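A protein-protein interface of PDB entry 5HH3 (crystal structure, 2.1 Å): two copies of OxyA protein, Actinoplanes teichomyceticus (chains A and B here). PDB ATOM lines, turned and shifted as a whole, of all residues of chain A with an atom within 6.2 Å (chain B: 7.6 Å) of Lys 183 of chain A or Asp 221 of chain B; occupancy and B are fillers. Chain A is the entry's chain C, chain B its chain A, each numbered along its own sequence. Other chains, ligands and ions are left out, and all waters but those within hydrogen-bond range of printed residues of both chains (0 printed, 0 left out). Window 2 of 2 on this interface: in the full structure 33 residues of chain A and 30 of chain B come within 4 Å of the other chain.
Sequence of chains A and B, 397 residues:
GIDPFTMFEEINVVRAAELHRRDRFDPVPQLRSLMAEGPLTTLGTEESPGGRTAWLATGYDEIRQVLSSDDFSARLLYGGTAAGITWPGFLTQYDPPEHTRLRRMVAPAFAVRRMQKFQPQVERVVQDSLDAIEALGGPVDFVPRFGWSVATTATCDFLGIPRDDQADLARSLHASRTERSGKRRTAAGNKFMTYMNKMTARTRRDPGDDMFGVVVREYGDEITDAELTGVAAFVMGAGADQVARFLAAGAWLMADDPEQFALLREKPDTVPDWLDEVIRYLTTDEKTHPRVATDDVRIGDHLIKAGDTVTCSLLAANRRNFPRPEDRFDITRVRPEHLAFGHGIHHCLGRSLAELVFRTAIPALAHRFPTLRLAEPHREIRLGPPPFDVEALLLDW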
ATOM      1  N   ARG A 180     -38.496  12.075 -14.630  1.00  0.00           N
ATOM      2  CA  ARG A 180     -37.821  11.033 -13.848  1.00  0.00           C
ATOM      3  C   ARG A 180     -36.468  10.743 -14.479  1.00  0.00           C
ATOM      4  O   ARG A 180     -35.450  10.723 -13.783  1.00  0.00           O
ATOM      5  CB  ARG A 180     -38.665   9.753 -13.797  1.00  0.00           C
ATOM      6  N   SER A 181     -36.480  10.513 -15.793  1.00  0.00           N
ATOM      7  CA  SER A 181     -35.256  10.375 -16.586  1.00  0.00           C
ATOM      8  C   SER A 181     -34.381  11.618 -16.406  1.00  0.00           C
ATOM      9  O   SER A 181     -34.808  12.726 -16.723  1.00  0.00           O
ATOM     10  CB  SER A 181     -35.600  10.194 -18.070  1.00  0.00           C
ATOM     11  OG  SER A 181     -34.443  10.223 -18.890  1.00  0.00           O
ATOM     12  N   GLY A 182     -33.171  11.434 -15.881  1.00  0.00           N
ATOM     13  CA  GLY A 182     -32.211  12.525 -15.740  1.00  0.00           C
ATOM     14  C   GLY A 182     -31.571  12.946 -17.064  1.00  0.00           C
ATOM     15  O   GLY A 182     -31.005  14.039 -17.141  1.00  0.00           O
ATOM     16  N   LYS A 183     -31.622  12.080 -18.089  1.00  0.00           N
ATOM     17  CA  LYS A 183     -31.148  12.435 -19.446  1.00  0.00           C
ATOM     18  C   LYS A 183     -32.011  13.499 -20.104  1.00  0.00           C
ATOM     19  O   LYS A 183     -31.496  14.482 -20.632  1.00  0.00           O
ATOM     20  CB  LYS A 183     -31.064  11.209 -20.371  1.00  0.00           C
ATOM     21  CG  LYS A 183     -29.670  10.632 -20.411  1.00  0.00           C
ATOM     22  CD  LYS A 183     -29.593   9.274 -21.084  1.00  0.00           C
ATOM     23  CE  LYS A 183     -28.158   8.759 -21.098  1.00  0.00           C
ATOM     24  NZ  LYS A 183     -27.547   8.719 -19.734  1.00  0.00           N
ATOM     25  N   ARG A 184     -33.321  13.296 -20.071  1.00  0.00           N
ATOM     26  CA  ARG A 184     -34.257  14.289 -20.587  1.00  0.00           C
ATOM     27  C   ARG A 184     -34.253  15.580 -19.744  1.00  0.00           C
ATOM     28  O   ARG A 184     -34.583  16.649 -20.251  1.00  0.00           O
ATOM     29  CB  ARG A 184     -35.666  13.714 -20.656  1.00  0.00           C
ATOM     30  CG  ARG A 184     -35.828  12.504 -21.566  1.00  0.00           C
ATOM     31  CD  ARG A 184     -37.282  12.065 -21.555  1.00  0.00           C
ATOM     32  NE  ARG A 184     -37.483  10.719 -22.088  1.00  0.00           N
ATOM     33  CZ  ARG A 184     -38.610  10.009 -21.972  1.00  0.00           C
ATOM     34  NH1 ARG A 184     -39.677  10.499 -21.330  1.00  0.00           N
ATOM     35  NH2 ARG A 184     -38.668   8.786 -22.500  1.00  0.00           N
ATOM     36  N   ARG A 185     -33.889  15.474 -18.465  1.00  0.00           N
ATOM     37  CA  ARG A 185     -33.667  16.657 -17.628  1.00  0.00           C
ATOM     38  C   ARG A 185     -32.544  17.560 -18.137  1.00  0.00           C
ATOM     39  O   ARG A 185     -32.724  18.780 -18.222  1.00  0.00           O
ATOM     40  CB  ARG A 185     -33.357  16.270 -16.182  1.00  0.00           C
ATOM     41  CG  ARG A 185     -34.582  15.949 -15.363  1.00  0.00           C
ATOM     42  CD  ARG A 185     -34.262  15.986 -13.887  1.00  0.00           C
ATOM     43  NE  ARG A 185     -35.488  15.829 -13.120  1.00  0.00           N
ATOM     44  CZ  ARG A 185     -35.650  16.182 -11.848  1.00  0.00           C
ATOM     45  NH1 ARG A 185     -34.656  16.727 -11.139  1.00  0.00           N
ATOM     46  NH2 ARG A 185     -36.834  15.990 -11.275  1.00  0.00           N
ATOM     47  N   THR A 186     -31.396  16.956 -18.445  1.00  0.00           N
ATOM     48  CA  THR A 186     -30.225  17.685 -18.955  1.00  0.00           C
ATOM     49  C   THR A 186     -30.438  18.246 -20.365  1.00  0.00           C
ATOM     50  O   THR A 186     -30.000  19.359 -20.652  1.00  0.00           O
ATOM     51  CB  THR A 186     -28.956  16.801 -18.981  1.00  0.00           C
ATOM     52  OG1 THR A 186     -29.218  15.607 -19.723  1.00  0.00           O
ATOM     53  CG2 THR A 186     -28.513  16.441 -17.570  1.00  0.00           C
ATOM     54  N   ALA A 187     -31.083  17.468 -21.236  1.00  0.00           N
ATOM     55  CA  ALA A 187     -31.420  17.914 -22.598  1.00  0.00           C
ATOM     56  C   ALA A 187     -32.370  19.122 -22.587  1.00  0.00           C
ATOM     57  O   ALA A 187     -32.150  20.103 -23.301  1.00  0.00           O
ATOM     58  CB  ALA A 187     -32.039  16.771 -23.389  1.00  0.00           C
ATOM     59  N   ALA A 188     -33.414  19.041 -21.768  1.00  0.00           N
ATOM     60  CA  ALA A 188     -34.375  20.127 -21.619  1.00  0.00           C
ATOM     61  C   ALA A 188     -33.751  21.368 -20.957  1.00  0.00           C
ATOM     62  O   ALA A 188     -34.010  22.500 -21.378  1.00  0.00           O
ATOM     63  CB  ALA A 188     -35.579  19.649 -20.816  1.00  0.00           C
ATOM     64  N   ARG B 101     -35.862   1.864 -10.328  1.00  0.00           N
ATOM     65  CA  ARG B 101     -34.943   2.636 -11.184  1.00  0.00           C
ATOM     66  C   ARG B 101     -33.698   3.085 -10.409  1.00  0.00           C
ATOM     67  O   ARG B 101     -32.580   2.920 -10.885  1.00  0.00           O
ATOM     68  CB  ARG B 101     -35.663   3.854 -11.799  1.00  0.00           C
ATOM     69  CG  ARG B 101     -34.758   4.893 -12.470  1.00  0.00           C
ATOM     70  CD  ARG B 101     -35.479   6.199 -12.802  1.00  0.00           C
ATOM     71  NE  ARG B 101     -34.538   7.314 -13.018  1.00  0.00           N
ATOM     72  CZ  ARG B 101     -33.963   8.053 -12.054  1.00  0.00           C
ATOM     73  NH1 ARG B 101     -34.207   7.828 -10.762  1.00  0.00           N
ATOM     74  NH2 ARG B 101     -33.128   9.053 -12.388  1.00  0.00           N
ATOM     75  N   MET B 105     -29.502   1.622 -10.509  1.00  0.00           N
ATOM     76  CA  MET B 105     -28.353   2.445 -10.859  1.00  0.00           C
ATOM     77  C   MET B 105     -27.194   2.380  -9.858  1.00  0.00           C
ATOM     78  O   MET B 105     -26.034   2.507 -10.263  1.00  0.00           O
ATOM     79  CB  MET B 105     -28.775   3.894 -11.095  1.00  0.00           C
ATOM     80  CG  MET B 105     -29.718   4.023 -12.270  1.00  0.00           C
ATOM     81  SD  MET B 105     -30.047   5.706 -12.797  1.00  0.00           S
ATOM     82  CE  MET B 105     -30.896   6.404 -11.390  1.00  0.00           C
ATOM     83  N   ARG B 204     -18.590  14.076 -11.571  1.00  0.00           N
ATOM     84  CA  ARG B 204     -19.215  14.437 -12.841  1.00  0.00           C
ATOM     85  C   ARG B 204     -18.190  14.901 -13.897  1.00  0.00           C
ATOM     86  O   ARG B 204     -18.311  14.565 -15.078  1.00  0.00           O
ATOM     87  CB  ARG B 204     -20.283  15.510 -12.600  1.00  0.00           C
ATOM     88  CG  ARG B 204     -21.324  15.611 -13.697  1.00  0.00           C
ATOM     89  CD  ARG B 204     -22.256  14.407 -13.732  1.00  0.00           C
ATOM     90  NE  ARG B 204     -23.311  14.429 -12.724  1.00  0.00           N
ATOM     91  CZ  ARG B 204     -24.271  13.510 -12.634  1.00  0.00           C
ATOM     92  NH1 ARG B 204     -25.205  13.613 -11.700  1.00  0.00           N
ATOM     93  NH2 ARG B 204     -24.312  12.479 -13.473  1.00  0.00           N
ATOM     94  N   VAL B 215     -20.996   4.485 -10.623  1.00  0.00           N
ATOM     95  CA  VAL B 215     -22.374   4.887 -10.923  1.00  0.00           C
ATOM     96  C   VAL B 215     -22.433   5.836 -12.135  1.00  0.00           C
ATOM     97  O   VAL B 215     -23.240   5.624 -13.040  1.00  0.00           O
ATOM     98  CB  VAL B 215     -23.074   5.533  -9.686  1.00  0.00           C
ATOM     99  CG1 VAL B 215     -24.457   6.067 -10.048  1.00  0.00           C
ATOM    100  CG2 VAL B 215     -23.187   4.535  -8.537  1.00  0.00           C
ATOM    101  N   VAL B 216     -21.572   6.863 -12.141  1.00  0.00           N
ATOM    102  CA  VAL B 216     -21.566   7.901 -13.188  1.00  0.00           C
ATOM    103  C   VAL B 216     -21.082   7.372 -14.543  1.00  0.00           C
ATOM    104  O   VAL B 216     -21.621   7.764 -15.579  1.00  0.00           O
ATOM    105  CB  VAL B 216     -20.762   9.160 -12.744  1.00  0.00           C
ATOM    106  CG1 VAL B 216     -20.559  10.158 -13.883  1.00  0.00           C
ATOM    107  CG2 VAL B 216     -21.492   9.847 -11.594  1.00  0.00           C
ATOM    108  N   GLU B 218     -21.458   4.214 -15.548  1.00  0.00           N
ATOM    109  CA  GLU B 218     -22.539   3.383 -16.075  1.00  0.00           C
ATOM    110  C   GLU B 218     -23.763   4.212 -16.508  1.00  0.00           C
ATOM    111  O   GLU B 218     -24.265   4.016 -17.611  1.00  0.00           O
ATOM    112  CB  GLU B 218     -22.934   2.260 -15.108  1.00  0.00           C
ATOM    113  CG  GLU B 218     -23.726   1.143 -15.797  1.00  0.00           C
ATOM    114  CD  GLU B 218     -23.767  -0.184 -15.037  1.00  0.00           C
ATOM    115  OE1 GLU B 218     -24.297  -1.167 -15.605  1.00  0.00           O
ATOM    116  OE2 GLU B 218     -23.289  -0.267 -13.882  1.00  0.00           O
ATOM    117  N   TYR B 219     -24.225   5.148 -15.673  1.00  0.00           N
ATOM    118  CA  TYR B 219     -25.509   5.837 -15.936  1.00  0.00           C
ATOM    119  C   TYR B 219     -25.424   7.313 -16.355  1.00  0.00           C
ATOM    120  O   TYR B 219     -26.254   7.782 -17.144  1.00  0.00           O
ATOM    121  CB  TYR B 219     -26.460   5.608 -14.766  1.00  0.00           C
ATOM    122  CG  TYR B 219     -26.872   4.158 -14.718  1.00  0.00           C
ATOM    123  CD1 TYR B 219     -27.890   3.683 -15.548  1.00  0.00           C
ATOM    124  CD2 TYR B 219     -26.210   3.245 -13.898  1.00  0.00           C
ATOM    125  CE1 TYR B 219     -28.259   2.346 -15.543  1.00  0.00           C
ATOM    126  CE2 TYR B 219     -26.569   1.899 -13.890  1.00  0.00           C
ATOM    127  CZ  TYR B 219     -27.599   1.459 -14.709  1.00  0.00           C
ATOM    128  OH  TYR B 219     -27.971   0.140 -14.715  1.00  0.00           O
ATOM    129  N   GLY B 220     -24.421   8.034 -15.863  1.00  0.00           N
ATOM    130  CA  GLY B 220     -24.101   9.351 -16.408  1.00  0.00           C
ATOM    131  C   GLY B 220     -25.173  10.351 -16.063  1.00  0.00           C
ATOM    132  O   GLY B 220     -25.443  10.571 -14.889  1.00  0.00           O
ATOM    133  N   ASP B 221     -25.801  10.947 -17.071  1.00  0.00           N
ATOM    134  CA  ASP B 221     -26.811  11.979 -16.792  1.00  0.00           C
ATOM    135  C   ASP B 221     -28.177  11.397 -16.412  1.00  0.00           C
ATOM    136  O   ASP B 221     -29.026  12.147 -15.943  1.00  0.00           O
ATOM    137  CB  ASP B 221     -26.912  13.102 -17.872  1.00  0.00           C
ATOM    138  CG  ASP B 221     -26.865  12.587 -19.310  1.00  0.00           C
ATOM    139  OD1 ASP B 221     -26.866  11.351 -19.517  1.00  0.00           O
ATOM    140  OD2 ASP B 221     -26.804  13.435 -20.234  1.00  0.00           O
ATOM    141  N   GLU B 222     -28.372  10.081 -16.551  1.00  0.00           N
ATOM    142  CA  GLU B 222     -29.596   9.432 -16.033  1.00  0.00           C
ATOM    143  C   GLU B 222     -29.851   9.652 -14.529  1.00  0.00           C
ATOM    144  O   GLU B 222     -30.982   9.871 -14.126  1.00  0.00           O
ATOM    145  CB  GLU B 222     -29.624   7.918 -16.336  1.00  0.00           C
ATOM    146  CG  GLU B 222     -30.579   7.529 -17.456  1.00  0.00           C
ATOM    147  CD  GLU B 222     -32.032   7.849 -17.136  1.00  0.00           C
ATOM    148  OE1 GLU B 222     -32.726   8.365 -18.039  1.00  0.00           O
ATOM    149  OE2 GLU B 222     -32.477   7.605 -15.988  1.00  0.00           O
ATOM    150  N   ILE B 223     -28.801   9.563 -13.718  1.00  0.00           N
ATOM    151  CA  ILE B 223     -28.885   9.847 -12.286  1.00  0.00           C
ATOM    152  C   ILE B 223     -28.568  11.338 -12.044  1.00  0.00           C
ATOM    153  O   ILE B 223     -27.598  11.882 -12.583  1.00  0.00           O
ATOM    154  CB  ILE B 223     -27.975   8.904 -11.453  1.00  0.00           C
ATOM    155  CG1 ILE B 223     -28.354   8.966  -9.971  1.00  0.00           C
ATOM    156  CG2 ILE B 223     -26.492   9.229 -11.635  1.00  0.00           C
ATOM    157  CD1 ILE B 223     -27.567   8.031  -9.080  1.00  0.00           C
ATOM    158  N   THR B 224     -29.391  11.998 -11.237  1.00  0.00           N
ATOM    159  CA  THR B 224     -29.256  13.443 -10.999  1.00  0.00           C
ATOM    160  C   THR B 224     -28.241  13.710  -9.885  1.00  0.00           C
ATOM    161  O   THR B 224     -27.871  12.792  -9.139  1.00  0.00           O
ATOM    162  CB  THR B 224     -30.609  14.063 -10.616  1.00  0.00           C
ATOM    163  OG1 THR B 224     -31.056  13.524  -9.360  1.00  0.00           O
ATOM    164  CG2 THR B 224     -31.658  13.772 -11.685  1.00  0.00           C
ATOM    165  N   ASP B 225     -27.789  14.958  -9.770  1.00  0.00           N
ATOM    166  CA  ASP B 225     -26.861  15.343  -8.699  1.00  0.00           C
ATOM    167  C   ASP B 225     -27.459  15.140  -7.294  1.00  0.00           C
ATOM    168  O   ASP B 225     -26.762  14.705  -6.368  1.00  0.00           O
ATOM    169  CB  ASP B 225     -26.397  16.793  -8.856  1.00  0.00           C
ATOM    170  CG  ASP B 225     -25.453  16.991 -10.047  1.00  0.00           C
ATOM    171  OD1 ASP B 225     -24.847  16.012 -10.544  1.00  0.00           O
ATOM    172  OD2 ASP B 225     -25.311  18.150 -10.474  1.00  0.00           O
ATOM    173  N   GLU B 227     -29.875  12.950  -6.434  1.00  0.00           N
ATOM    174  CA  GLU B 227     -29.879  11.512  -6.222  1.00  0.00           C
ATOM    175  C   GLU B 227     -28.500  10.982  -5.836  1.00  0.00           C
ATOM    176  O   GLU B 227     -28.376  10.239  -4.874  1.00  0.00           O
ATOM    177  CB  GLU B 227     -30.384  10.778  -7.456  1.00  0.00           C
ATOM    178  CG  GLU B 227     -31.873  10.932  -7.701  1.00  0.00           C
ATOM    179  CD  GLU B 227     -32.311  10.388  -9.049  1.00  0.00           C
ATOM    180  OE1 GLU B 227     -31.515  10.425 -10.016  1.00  0.00           O
ATOM    181  OE2 GLU B 227     -33.466   9.916  -9.146  1.00  0.00           O
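N of Arg 184 of chain A is in hydrogen-bond range of OG of Ser 181 of chain A (3.5 Å).
OG1 of Thr 186 of chain A sits at hydrogen-bond distance from O of Lys 183 of chain A (2.7 Å).
OE2 of Glu 222 of chain B is in salt-bridge range of NE of Arg 101 of chain B.
OG of Ser 181 of chain A sits close to N of Lys 183 of chain A (3.5 Å).
The side-chain carboxylate (OE2) of Glu 227 of chain B is in salt-bridge range of the guanidinium group (NH1) of Arg 101 of chain B.
Of the 9 printed residues of chain A, 5 touch a printed residue of chain B.
Among the printed residues, Asp or Glu carboxylates within 4 Å of a Lys or Arg side-chain nitrogen of the other chain: Lys 183 of chain A with Asp 221 of chain B (2.7 Å).
No position is printed for both chains.
Of the 8 pairs that touch across the chains among the printed residues, none has its exchanged pair printed and touching as well.
The backbone NH (N) of Gly 182 of chain A lies within hydrogen-bond range of the backbone carbonyl oxygen (O) of Glu 222 of chain B.
The side-chain hydroxyl (OG1) of Thr 186 of chain A lies within hydrogen-bond range of the side-chain carboxylate (OD2) of Asp 221 of chain B (3.3 Å).
The guanidinium group (NH2) of Arg 101 of chain B lies within hydrogen-bond range of the backbone carbonyl oxygen (O) of Arg 180 of chain A, at 3.2 Å.
O of Tyr 219 of chain B lies within hydrogen-bond range of NZ of Lys 183 of chain A, 3.0 Å away.
The side-chain carboxylate (OD1) of Asp 221 of chain B is in salt-bridge range of the side-chain amino group (NZ) of Lys 183 of chain A, 2.7 Å away.
The backbone carbonyl oxygen (O) of Gly 182 of chain A sits close to the backbone carbonyl oxygen (O) of Asp 221 of chain B (3.0 Å).
The side-chain carboxylate of Glu 222 of chain B lies within hydrogen-bond range of the side-chain hydroxyl of Ser 181 of chain A (2.7 Å).
Lys 183 of chain A touches Glu 222 of chain B (NZ to N, 3.6 Å).
Gly 182 of chain A touches two residues of chain B.
Lys 183 of chain A touches just these residues of chain B: Tyr 219, Asp 221 and Glu 222.
Printed residues of chain A within 4 Å of Arg 101 of chain B: Arg 180.
Of chain A, only Gly 182 (2.9 Å), Lys 183 (2.7 Å) and Thr 186 (3.3 Å) come within 4 Å of Asp 221 of chain B.
Printed residues of chain A within 4 Å of Glu 222 of chain B: Ser 181 (2.7 Å), Gly 182 (3.2 Å) and Lys 183 (3.6 Å).
The nearest printed residue of chain A that does not touch Asp 221 of chain B is Ser 181 of chain A (5.4 Å).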
